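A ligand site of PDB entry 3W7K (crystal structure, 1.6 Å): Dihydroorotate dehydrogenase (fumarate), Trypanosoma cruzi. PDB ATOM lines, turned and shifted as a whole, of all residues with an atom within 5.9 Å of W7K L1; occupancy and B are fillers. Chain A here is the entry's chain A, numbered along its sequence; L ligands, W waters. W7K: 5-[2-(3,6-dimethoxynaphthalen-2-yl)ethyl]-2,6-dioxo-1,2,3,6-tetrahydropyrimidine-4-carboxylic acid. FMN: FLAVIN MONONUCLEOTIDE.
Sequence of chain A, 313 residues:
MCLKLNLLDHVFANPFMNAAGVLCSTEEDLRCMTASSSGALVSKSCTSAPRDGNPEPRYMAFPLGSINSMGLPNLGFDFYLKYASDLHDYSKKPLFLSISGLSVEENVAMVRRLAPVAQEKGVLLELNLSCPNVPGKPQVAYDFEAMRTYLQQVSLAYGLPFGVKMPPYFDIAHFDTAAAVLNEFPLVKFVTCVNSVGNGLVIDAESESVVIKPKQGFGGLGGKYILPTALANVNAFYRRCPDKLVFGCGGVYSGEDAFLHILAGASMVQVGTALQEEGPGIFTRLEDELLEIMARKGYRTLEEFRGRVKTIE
O of Met 70 lies within hydrogen-bond range of N of Asn 54, 2.8 Å away. The side-chain amide oxygen (OD1) of Asn 128 is in hydrogen-bond range of the side-chain amide nitrogen (ND2) of Asn 195 (3.4 Å). N of Gly 220 lies within hydrogen-bond range of O of Asn 68 (2.8 Å). OD1 of Asn 195 is in hydrogen-bond range of OG of Ser 196, 3.4 Å away. The side-chain amide oxygen (OD1) of Asn 128 sits at hydrogen-bond distance from the backbone NH (N) of Ser 130 (3.0 Å). The side-chain amide oxygen of Asn 68 is in hydrogen-bond range of the backbone NH of Met 70, 3.2 Å away. O of Leu 72 is in hydrogen-bond range of NE of Arg 51 (3.3 Å). The backbone carbonyl oxygen of Gly 71 sits at hydrogen-bond distance from the guanidinium group of Arg 51 (2.9 Å).
The backbone carbonyl oxygen (O) of Ser 130 lies close to an oxygen (OAE) of W7K L1 (3.4 Å). Merely in contact with W7K L1: Pro 132 (3.8 Å). Within 4 Å of W7K L1: Lys 44, Asn 54, Asn 68, Met 70, Gly 71, Leu 72, Asn 128, Ser 130, Pro 132, Asn 195 and Ser 196.
The side-chain amide nitrogen (ND2) of Asn 54 lies within hydrogen-bond range of an oxygen (OAP) of W7K L1 (3.4 Å). The side-chain amide nitrogen of Asn 195 is in hydrogen-bond range of an oxygen (O2) of FMN L2, 3.4 Å away. OAF of W7K L1 is in hydrogen-bond range of N of Met 70. N3 of FMN L2 is in hydrogen-bond range of OG of Ser 45, 2.7 Å away. OAD of W7K L1 is in hydrogen-bond range of ND2 of Asn 68, 2.9 Å away. An oxygen (OAC) of W7K L1 is in hydrogen-bond range of the backbone NH (N) of Leu 72 (2.9 Å). The backbone NH of Gly 71 sits at hydrogen-bond distance from an oxygen (OAF) of W7K L1, at 2.8 Å. NZ of Lys 165 is in hydrogen-bond range of O2' of FMN L2, 2.9 Å away. OAD of W7K L1 lies within hydrogen-bond range of OG of Ser 196 (2.8 Å). OAC of W7K L1 is in salt-bridge range of NZ of Lys 44, at 3.0 Å. The side-chain amide oxygen (OD1) of Asn 195 is in hydrogen-bond range of a nitrogen (NAO) of W7K L1, at 2.7 Å. An oxygen (O2) of FMN L2 lies within hydrogen-bond range of the side-chain amide nitrogen (ND2) of Asn 128, at 3.3 Å. The side-chain amide nitrogen (ND2) of Asn 128 sits at hydrogen-bond distance from an oxygen (OAE) of W7K L1. The side-chain amino group of Lys 44 lies within hydrogen-bond range of an oxygen (O4) of FMN L2.
Water W2 bridges the side-chain amide oxygen of Asn 68 (3.0 Å) and an oxygen (OAF) of W7K L1 (3.0 Å).
A nitrogen (N1) of FMN L2 lies close to a nitrogen (NAO) of W7K L1 (3.4 Å).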
ATOM      1  N   LYS A  44     -22.462 -15.363   9.990  1.00  0.00           N
ATOM      2  CA  LYS A  44     -22.033 -16.335  10.927  1.00  0.00           C
ATOM      3  C   LYS A  44     -21.816 -15.701  12.262  1.00  0.00           C
ATOM      4  O   LYS A  44     -21.136 -14.705  12.349  1.00  0.00           O
ATOM      5  CB  LYS A  44     -20.792 -17.033  10.462  1.00  0.00           C
ATOM      6  CG  LYS A  44     -20.167 -17.935  11.488  1.00  0.00           C
ATOM      7  CD  LYS A  44     -20.930 -19.213  11.850  1.00  0.00           C
ATOM      8  CE  LYS A  44     -20.437 -19.938  13.130  1.00  0.00           C
ATOM      9  NZ  LYS A  44     -21.257 -21.178  13.453  1.00  0.00           N
ATOM     10  N   SER A  45     -22.347 -16.325  13.288  1.00  0.00           N
ATOM     11  CA  SER A  45     -22.119 -15.829  14.685  1.00  0.00           C
ATOM     12  C   SER A  45     -20.618 -15.713  14.857  1.00  0.00           C
ATOM     13  O   SER A  45     -19.894 -16.618  14.592  1.00  0.00           O
ATOM     14  CB  SER A  45     -22.673 -16.714  15.762  1.00  0.00           C
ATOM     15  OG  SER A  45     -24.073 -16.730  15.721  1.00  0.00           O
ATOM     16  N   ARG A  51     -11.779 -18.092  14.788  1.00  0.00           N
ATOM     17  CA  ARG A  51     -11.756 -19.433  15.352  1.00  0.00           C
ATOM     18  C   ARG A  51     -11.782 -20.482  14.248  1.00  0.00           C
ATOM     19  O   ARG A  51     -12.492 -20.336  13.285  1.00  0.00           O
ATOM     20  CB  ARG A  51     -12.943 -19.734  16.281  1.00  0.00           C
ATOM     21  CG  ARG A  51     -13.108 -18.836  17.468  1.00  0.00           C
ATOM     22  CD  ARG A  51     -14.386 -19.121  18.195  1.00  0.00           C
ATOM     23  NE  ARG A  51     -14.732 -20.515  18.512  1.00  0.00           N
ATOM     24  CZ  ARG A  51     -14.472 -21.107  19.649  1.00  0.00           C
ATOM     25  NH1 ARG A  51     -13.744 -20.460  20.616  1.00  0.00           N
ATOM     26  NH2 ARG A  51     -14.872 -22.356  19.864  1.00  0.00           N
ATOM     27  N   ASN A  54     -14.411 -26.710  15.874  1.00  0.00           N
ATOM     28  CA  ASN A  54     -14.145 -28.085  16.362  1.00  0.00           C
ATOM     29  C   ASN A  54     -13.581 -29.005  15.281  1.00  0.00           C
ATOM     30  O   ASN A  54     -13.697 -28.744  14.097  1.00  0.00           O
ATOM     31  CB  ASN A  54     -15.441 -28.617  16.906  1.00  0.00           C
ATOM     32  CG  ASN A  54     -15.834 -28.039  18.244  1.00  0.00           C
ATOM     33  OD1 ASN A  54     -15.002 -27.434  18.979  1.00  0.00           O
ATOM     34  ND2 ASN A  54     -17.089 -28.212  18.618  1.00  0.00           N
ATOM     35  N   ASN A  68     -24.933 -31.022  14.411  1.00  0.00           N
ATOM     36  CA  ASN A  68     -23.702 -30.266  14.299  1.00  0.00           C
ATOM     37  C   ASN A  68     -23.068 -29.992  15.613  1.00  0.00           C
ATOM     38  O   ASN A  68     -23.741 -29.710  16.605  1.00  0.00           O
ATOM     39  CB  ASN A  68     -23.854 -28.968  13.491  1.00  0.00           C
ATOM     40  CG  ASN A  68     -24.289 -27.810  14.337  1.00  0.00           C
ATOM     41  OD1 ASN A  68     -23.446 -27.117  14.960  1.00  0.00           O
ATOM     42  ND2 ASN A  68     -25.588 -27.494  14.398  1.00  0.00           N
ATOM     43  N   SER A  69     -21.738 -29.961  15.596  1.00  0.00           N
ATOM     44  CA  SER A  69     -20.964 -29.376  16.706  1.00  0.00           C
ATOM     45  C   SER A  69     -19.862 -28.567  16.055  1.00  0.00           C
ATOM     46  O   SER A  69     -18.665 -28.859  16.155  1.00  0.00           O
ATOM     47  CB  SER A  69     -20.401 -30.453  17.638  1.00  0.00           C
ATOM     48  OG  SER A  69     -19.735 -29.804  18.721  1.00  0.00           O
ATOM     49  N   MET A  70     -20.278 -27.524  15.330  1.00  0.00           N
ATOM     50  CA  MET A  70     -19.313 -26.749  14.592  1.00  0.00           C
ATOM     51  C   MET A  70     -18.241 -26.114  15.483  1.00  0.00           C
ATOM     52  O   MET A  70     -17.053 -26.046  15.130  1.00  0.00           O
ATOM     53  CB  MET A  70     -19.992 -25.657  13.806  1.00  0.00           C
ATOM     54  CG  MET A  70     -21.038 -26.026  12.772  1.00  0.00           C
ATOM     55  SD  MET A  70     -20.504 -27.262  11.588  1.00  0.00           S
ATOM     56  CE  MET A  70     -19.443 -26.324  10.659  1.00  0.00           C
ATOM     57  N   GLY A  71     -18.632 -25.557  16.638  1.00  0.00           N
ATOM     58  CA  GLY A  71     -17.701 -24.902  17.518  1.00  0.00           C
ATOM     59  C   GLY A  71     -17.389 -23.457  17.209  1.00  0.00           C
ATOM     60  O   GLY A  71     -16.259 -23.005  17.401  1.00  0.00           O
ATOM     61  N   LEU A  72     -18.333 -22.764  16.563  1.00  0.00           N
ATOM     62  CA  LEU A  72     -18.219 -21.347  16.212  1.00  0.00           C
ATOM     63  C   LEU A  72     -16.938 -21.077  15.344  1.00  0.00           C
ATOM     64  O   LEU A  72     -16.200 -20.106  15.554  1.00  0.00           O
ATOM     65  CB  LEU A  72     -18.183 -20.463  17.472  1.00  0.00           C
ATOM     66  CG  LEU A  72     -18.892 -19.162  17.670  1.00  0.00           C
ATOM     67  CD1 LEU A  72     -20.285 -19.080  17.071  1.00  0.00           C
ATOM     68  CD2 LEU A  72     -18.917 -18.919  19.226  1.00  0.00           C
ATOM     69  N   PRO A  73     -16.668 -21.866  14.306  1.00  0.00           N
ATOM     70  CA  PRO A  73     -15.630 -21.476  13.326  1.00  0.00           C
ATOM     71  C   PRO A  73     -16.086 -20.148  12.668  1.00  0.00           C
ATOM     72  O   PRO A  73     -17.256 -20.021  12.243  1.00  0.00           O
ATOM     73  CB  PRO A  73     -15.619 -22.594  12.325  1.00  0.00           C
ATOM     74  CG  PRO A  73     -16.948 -23.202  12.368  1.00  0.00           C
ATOM     75  CD  PRO A  73     -17.573 -22.887  13.752  1.00  0.00           C
ATOM     76  N   SER A 100     -21.673 -13.880  18.932  1.00  0.00           N
ATOM     77  CA  SER A 100     -21.681 -14.935  19.924  1.00  0.00           C
ATOM     78  C   SER A 100     -20.416 -15.013  20.732  1.00  0.00           C
ATOM     79  O   SER A 100     -19.744 -16.071  20.813  1.00  0.00           O
ATOM     80  CB  SER A 100     -22.062 -16.252  19.237  1.00  0.00           C
ATOM     81  OG  SER A 100     -22.084 -17.293  20.112  1.00  0.00           O
ATOM     82  N   ASN A 128     -26.620 -13.967  19.838  1.00  0.00           N
ATOM     83  CA  ASN A 128     -26.802 -15.340  20.116  1.00  0.00           C
ATOM     84  C   ASN A 128     -26.713 -15.703  21.570  1.00  0.00           C
ATOM     85  O   ASN A 128     -25.657 -15.654  22.131  1.00  0.00           O
ATOM     86  CB  ASN A 128     -25.797 -16.139  19.302  1.00  0.00           C
ATOM     87  CG  ASN A 128     -26.106 -17.617  19.320  1.00  0.00           C
ATOM     88  OD1 ASN A 128     -27.045 -18.081  19.892  1.00  0.00           O
ATOM     89  ND2 ASN A 128     -25.259 -18.331  18.606  1.00  0.00           N
ATOM     90  N   SER A 130     -28.037 -18.634  22.718  1.00  0.00           N
ATOM     91  CA  SER A 130     -27.894 -20.064  22.798  1.00  0.00           C
ATOM     92  C   SER A 130     -26.483 -20.375  22.401  1.00  0.00           C
ATOM     93  O   SER A 130     -26.086 -20.851  21.330  1.00  0.00           O
ATOM     94  CB  SER A 130     -28.918 -20.813  21.927  1.00  0.00           C
ATOM     95  OG  SER A 130     -28.460 -22.115  21.621  1.00  0.00           O
ATOM     96  N   CYS A 131     -25.664 -20.192  23.454  1.00  0.00           N
ATOM     97  CA  CYS A 131     -24.302 -20.150  23.264  1.00  0.00           C
ATOM     98  C   CYS A 131     -23.614 -20.504  24.661  1.00  0.00           C
ATOM     99  O   CYS A 131     -24.098 -20.057  25.709  1.00  0.00           O
ATOM    100  CB  CYS A 131     -24.093 -18.629  23.057  1.00  0.00           C
ATOM    101  SG  CYS A 131     -22.366 -18.106  23.026  1.00  0.00           S
ATOM    102  N   PRO A 132     -22.425 -21.080  24.671  1.00  0.00           N
ATOM    103  CA  PRO A 132     -21.672 -21.250  25.919  1.00  0.00           C
ATOM    104  C   PRO A 132     -21.269 -20.054  26.783  1.00  0.00           C
ATOM    105  O   PRO A 132     -20.895 -19.004  26.374  1.00  0.00           O
ATOM    106  CB  PRO A 132     -20.362 -21.892  25.421  1.00  0.00           C
ATOM    107  CG  PRO A 132     -20.252 -21.439  24.000  1.00  0.00           C
ATOM    108  CD  PRO A 132     -21.671 -21.682  23.563  1.00  0.00           C
ATOM    109  N   LYS A 165     -31.256 -14.438  19.514  1.00  0.00           N
ATOM    110  CA  LYS A 165     -31.489 -15.825  19.029  1.00  0.00           C
ATOM    111  C   LYS A 165     -31.590 -16.715  20.225  1.00  0.00           C
ATOM    112  O   LYS A 165     -30.672 -16.791  21.060  1.00  0.00           O
ATOM    113  CB  LYS A 165     -30.334 -16.267  18.167  1.00  0.00           C
ATOM    114  CG  LYS A 165     -30.404 -17.713  17.614  1.00  0.00           C
ATOM    115  CD  LYS A 165     -31.353 -17.897  16.468  1.00  0.00           C
ATOM    116  CE  LYS A 165     -31.169 -19.220  15.784  1.00  0.00           C
ATOM    117  NZ  LYS A 165     -29.986 -19.293  14.967  1.00  0.00           N
ATOM    118  N   ASN A 195     -32.848 -21.725  17.914  1.00  0.00           N
ATOM    119  CA  ASN A 195     -31.518 -22.405  17.656  1.00  0.00           C
ATOM    120  C   ASN A 195     -31.722 -23.939  17.619  1.00  0.00           C
ATOM    121  O   ASN A 195     -32.867 -24.456  17.858  1.00  0.00           O
ATOM    122  CB  ASN A 195     -30.511 -21.938  18.733  1.00  0.00           C
ATOM    123  CG  ASN A 195     -29.108 -21.860  18.187  1.00  0.00           C
ATOM    124  OD1 ASN A 195     -28.638 -22.777  17.581  1.00  0.00           O
ATOM    125  ND2 ASN A 195     -28.461 -20.727  18.354  1.00  0.00           N
ATOM    126  N   SER A 196     -30.634 -24.680  17.370  1.00  0.00           N
ATOM    127  CA  SER A 196     -30.707 -26.136  17.343  1.00  0.00           C
ATOM    128  C   SER A 196     -31.164 -26.707  18.643  1.00  0.00           C
ATOM    129  O   SER A 196     -31.028 -26.110  19.721  1.00  0.00           O
ATOM    130  CB  SER A 196     -29.350 -26.665  16.826  1.00  0.00           C
ATOM    131  OG  SER A 196     -28.378 -26.157  17.653  1.00  0.00           O
ATOM    132  N   LYS A 215     -17.296 -33.886  21.107  1.00  0.00           N
ATOM    133  CA  LYS A 215     -18.218 -34.117  22.221  1.00  0.00           C
ATOM    134  C   LYS A 215     -18.865 -35.530  22.177  1.00  0.00           C
ATOM    135  O   LYS A 215     -20.029 -35.723  22.459  1.00  0.00           O
ATOM    136  CB  LYS A 215     -19.311 -33.025  22.283  1.00  0.00           C
ATOM    137  CG  LYS A 215     -18.720 -31.640  22.524  1.00  0.00           C
ATOM    138  CD  LYS A 215     -17.913 -31.566  23.824  1.00  0.00           C
ATOM    139  CE  LYS A 215     -16.806 -30.526  23.742  1.00  0.00           C
ATOM    140  NZ  LYS A 215     -16.749 -29.678  24.957  1.00  0.00           N
ATOM    141  N   GLY A 220     -26.027 -30.262  18.167  1.00  0.00           N
ATOM    142  CA  GLY A 220     -27.368 -29.694  18.062  1.00  0.00           C
ATOM    143  C   GLY A 220     -28.103 -30.201  16.825  1.00  0.00           C
ATOM    144  O   GLY A 220     -27.513 -30.368  15.731  1.00  0.00           O
HETATM  145  OAC W7K L   1     -21.185 -22.805  16.012  1.00  0.00           O
HETATM  146  CAR W7K L   1     -21.878 -23.704  16.528  1.00  0.00           C
HETATM  147  OAF W7K L   1     -21.343 -24.771  16.895  1.00  0.00           O
HETATM  148  CAV W7K L   1     -23.246 -23.522  16.703  1.00  0.00           C
HETATM  149  NAN W7K L   1     -24.149 -24.509  16.280  1.00  0.00           N
HETATM  150  CAX W7K L   1     -25.519 -24.318  16.451  1.00  0.00           C
HETATM  151  OAD W7K L   1     -26.315 -25.182  16.079  1.00  0.00           O
HETATM  152  NAO W7K L   1     -25.994 -23.149  17.052  1.00  0.00           N
HETATM  153  CAY W7K L   1     -25.092 -22.162  17.475  1.00  0.00           C
HETATM  154  OAE W7K L   1     -25.511 -21.133  18.005  1.00  0.00           O
HETATM  155  CAW W7K L   1     -23.724 -22.357  17.295  1.00  0.00           C
HETATM  156  CAM W7K L   1     -22.819 -21.379  17.722  1.00  0.00           C
HETATM  157  CAL W7K L   1     -22.753 -21.393  19.254  1.00  0.00           C
HETATM  158  CAT W7K L   1     -22.089 -22.529  19.680  1.00  0.00           C
HETATM  159  CAJ W7K L   1     -20.713 -22.495  19.933  1.00  0.00           C
HETATM  160  CAZ W7K L   1     -20.057 -23.641  20.366  1.00  0.00           C
HETATM  161  CAH W7K L   1     -18.692 -23.599  20.617  1.00  0.00           C
HETATM  162  CAG W7K L   1     -18.027 -24.745  21.047  1.00  0.00           C
HETATM  163  CAS W7K L   1     -18.728 -25.922  21.221  1.00  0.00           C
HETATM  164  OAP W7K L   1     -18.079 -27.041  21.643  1.00  0.00           O
HETATM  165  CAA W7K L   1     -16.684 -26.778  21.748  1.00  0.00           C
HETATM  166  CAI W7K L   1     -20.103 -25.965  20.972  1.00  0.00           C
HETATM  167  CBA W7K L   1     -20.756 -24.828  20.544  1.00  0.00           C
HETATM  168  CAK W7K L   1     -22.131 -24.870  20.295  1.00  0.00           C
HETATM  169  CAU W7K L   1     -22.777 -23.723  19.859  1.00  0.00           C
HETATM  170  OAQ W7K L   1     -24.109 -23.695  19.600  1.00  0.00           O
HETATM  171  CAB W7K L   1     -24.741 -24.814  20.217  1.00  0.00           C
HETATM  172  N1  FMN L   2     -27.150 -20.589  15.115  1.00  0.00           N
HETATM  173  C2  FMN L   2     -26.593 -19.434  15.485  1.00  0.00           C
HETATM  174  O2  FMN L   2     -27.351 -18.595  16.006  1.00  0.00           O
HETATM  175  N3  FMN L   2     -25.326 -19.120  15.200  1.00  0.00           N
HETATM  176  C4  FMN L   2     -24.518 -19.976  14.484  1.00  0.00           C
HETATM  177  O4  FMN L   2     -23.344 -19.638  14.175  1.00  0.00           O
HETATM  178  C4A FMN L   2     -25.023 -21.243  14.109  1.00  0.00           C
HETATM  179  N5  FMN L   2     -24.267 -22.099  13.393  1.00  0.00           N
HETATM  180  C5A FMN L   2     -24.857 -23.205  12.815  1.00  0.00           C
HETATM  181  C6  FMN L   2     -24.136 -23.996  11.930  1.00  0.00           C
HETATM  182  C7  FMN L   2     -24.674 -25.122  11.382  1.00  0.00           C
HETATM  183  C7M FMN L   2     -23.896 -25.954  10.423  1.00  0.00           C
HETATM  184  C8  FMN L   2     -26.062 -25.381  11.625  1.00  0.00           C
HETATM  185  C8M FMN L   2     -26.696 -26.552  11.020  1.00  0.00           C
HETATM  186  C9  FMN L   2     -26.804 -24.572  12.484  1.00  0.00           C
HETATM  187  C9A FMN L   2     -26.232 -23.487  13.100  1.00  0.00           C
HETATM  188  N10 FMN L   2     -26.978 -22.647  13.956  1.00  0.00           N
HETATM  189  C10 FMN L   2     -26.421 -21.450  14.375  1.00  0.00           C
HETATM  190  C1' FMN L   2     -28.379 -22.922  14.221  1.00  0.00           C
HETATM  191  C2' FMN L   2     -29.256 -22.552  13.010  1.00  0.00           C
HETATM  192  O2' FMN L   2     -29.163 -21.120  12.918  1.00  0.00           O
HETATM  193  C3' FMN L   2     -30.694 -22.899  13.306  1.00  0.00           C
HETATM  194  O3' FMN L   2     -31.155 -22.178  14.491  1.00  0.00           O
HETATM  195  C4' FMN L   2     -30.911 -24.436  13.478  1.00  0.00           C
HETATM  196  O4' FMN L   2     -30.081 -25.130  12.531  1.00  0.00           O
HETATM  197  C5' FMN L   2     -32.406 -24.747  13.261  1.00  0.00           C
HETATM  198  O5' FMN L   2     -32.875 -24.411  11.968  1.00  0.00           O
HETATM  199  P   FMN L   2     -33.077 -25.600  10.859  1.00  0.00           P
HETATM  200  O1P FMN L   2     -33.531 -24.836   9.653  1.00  0.00           O
HETATM  201  O2P FMN L   2     -34.003 -26.605  11.402  1.00  0.00           O
HETATM  202  O3P FMN L   2     -31.664 -26.217  10.654  1.00  0.00           O
HETATM  203  O   HOH W   1     -27.392 -26.688  20.207  1.00  0.00           O
HETATM  204  O   HOH W   2     -23.159 -26.986  17.923  1.00  0.00           O
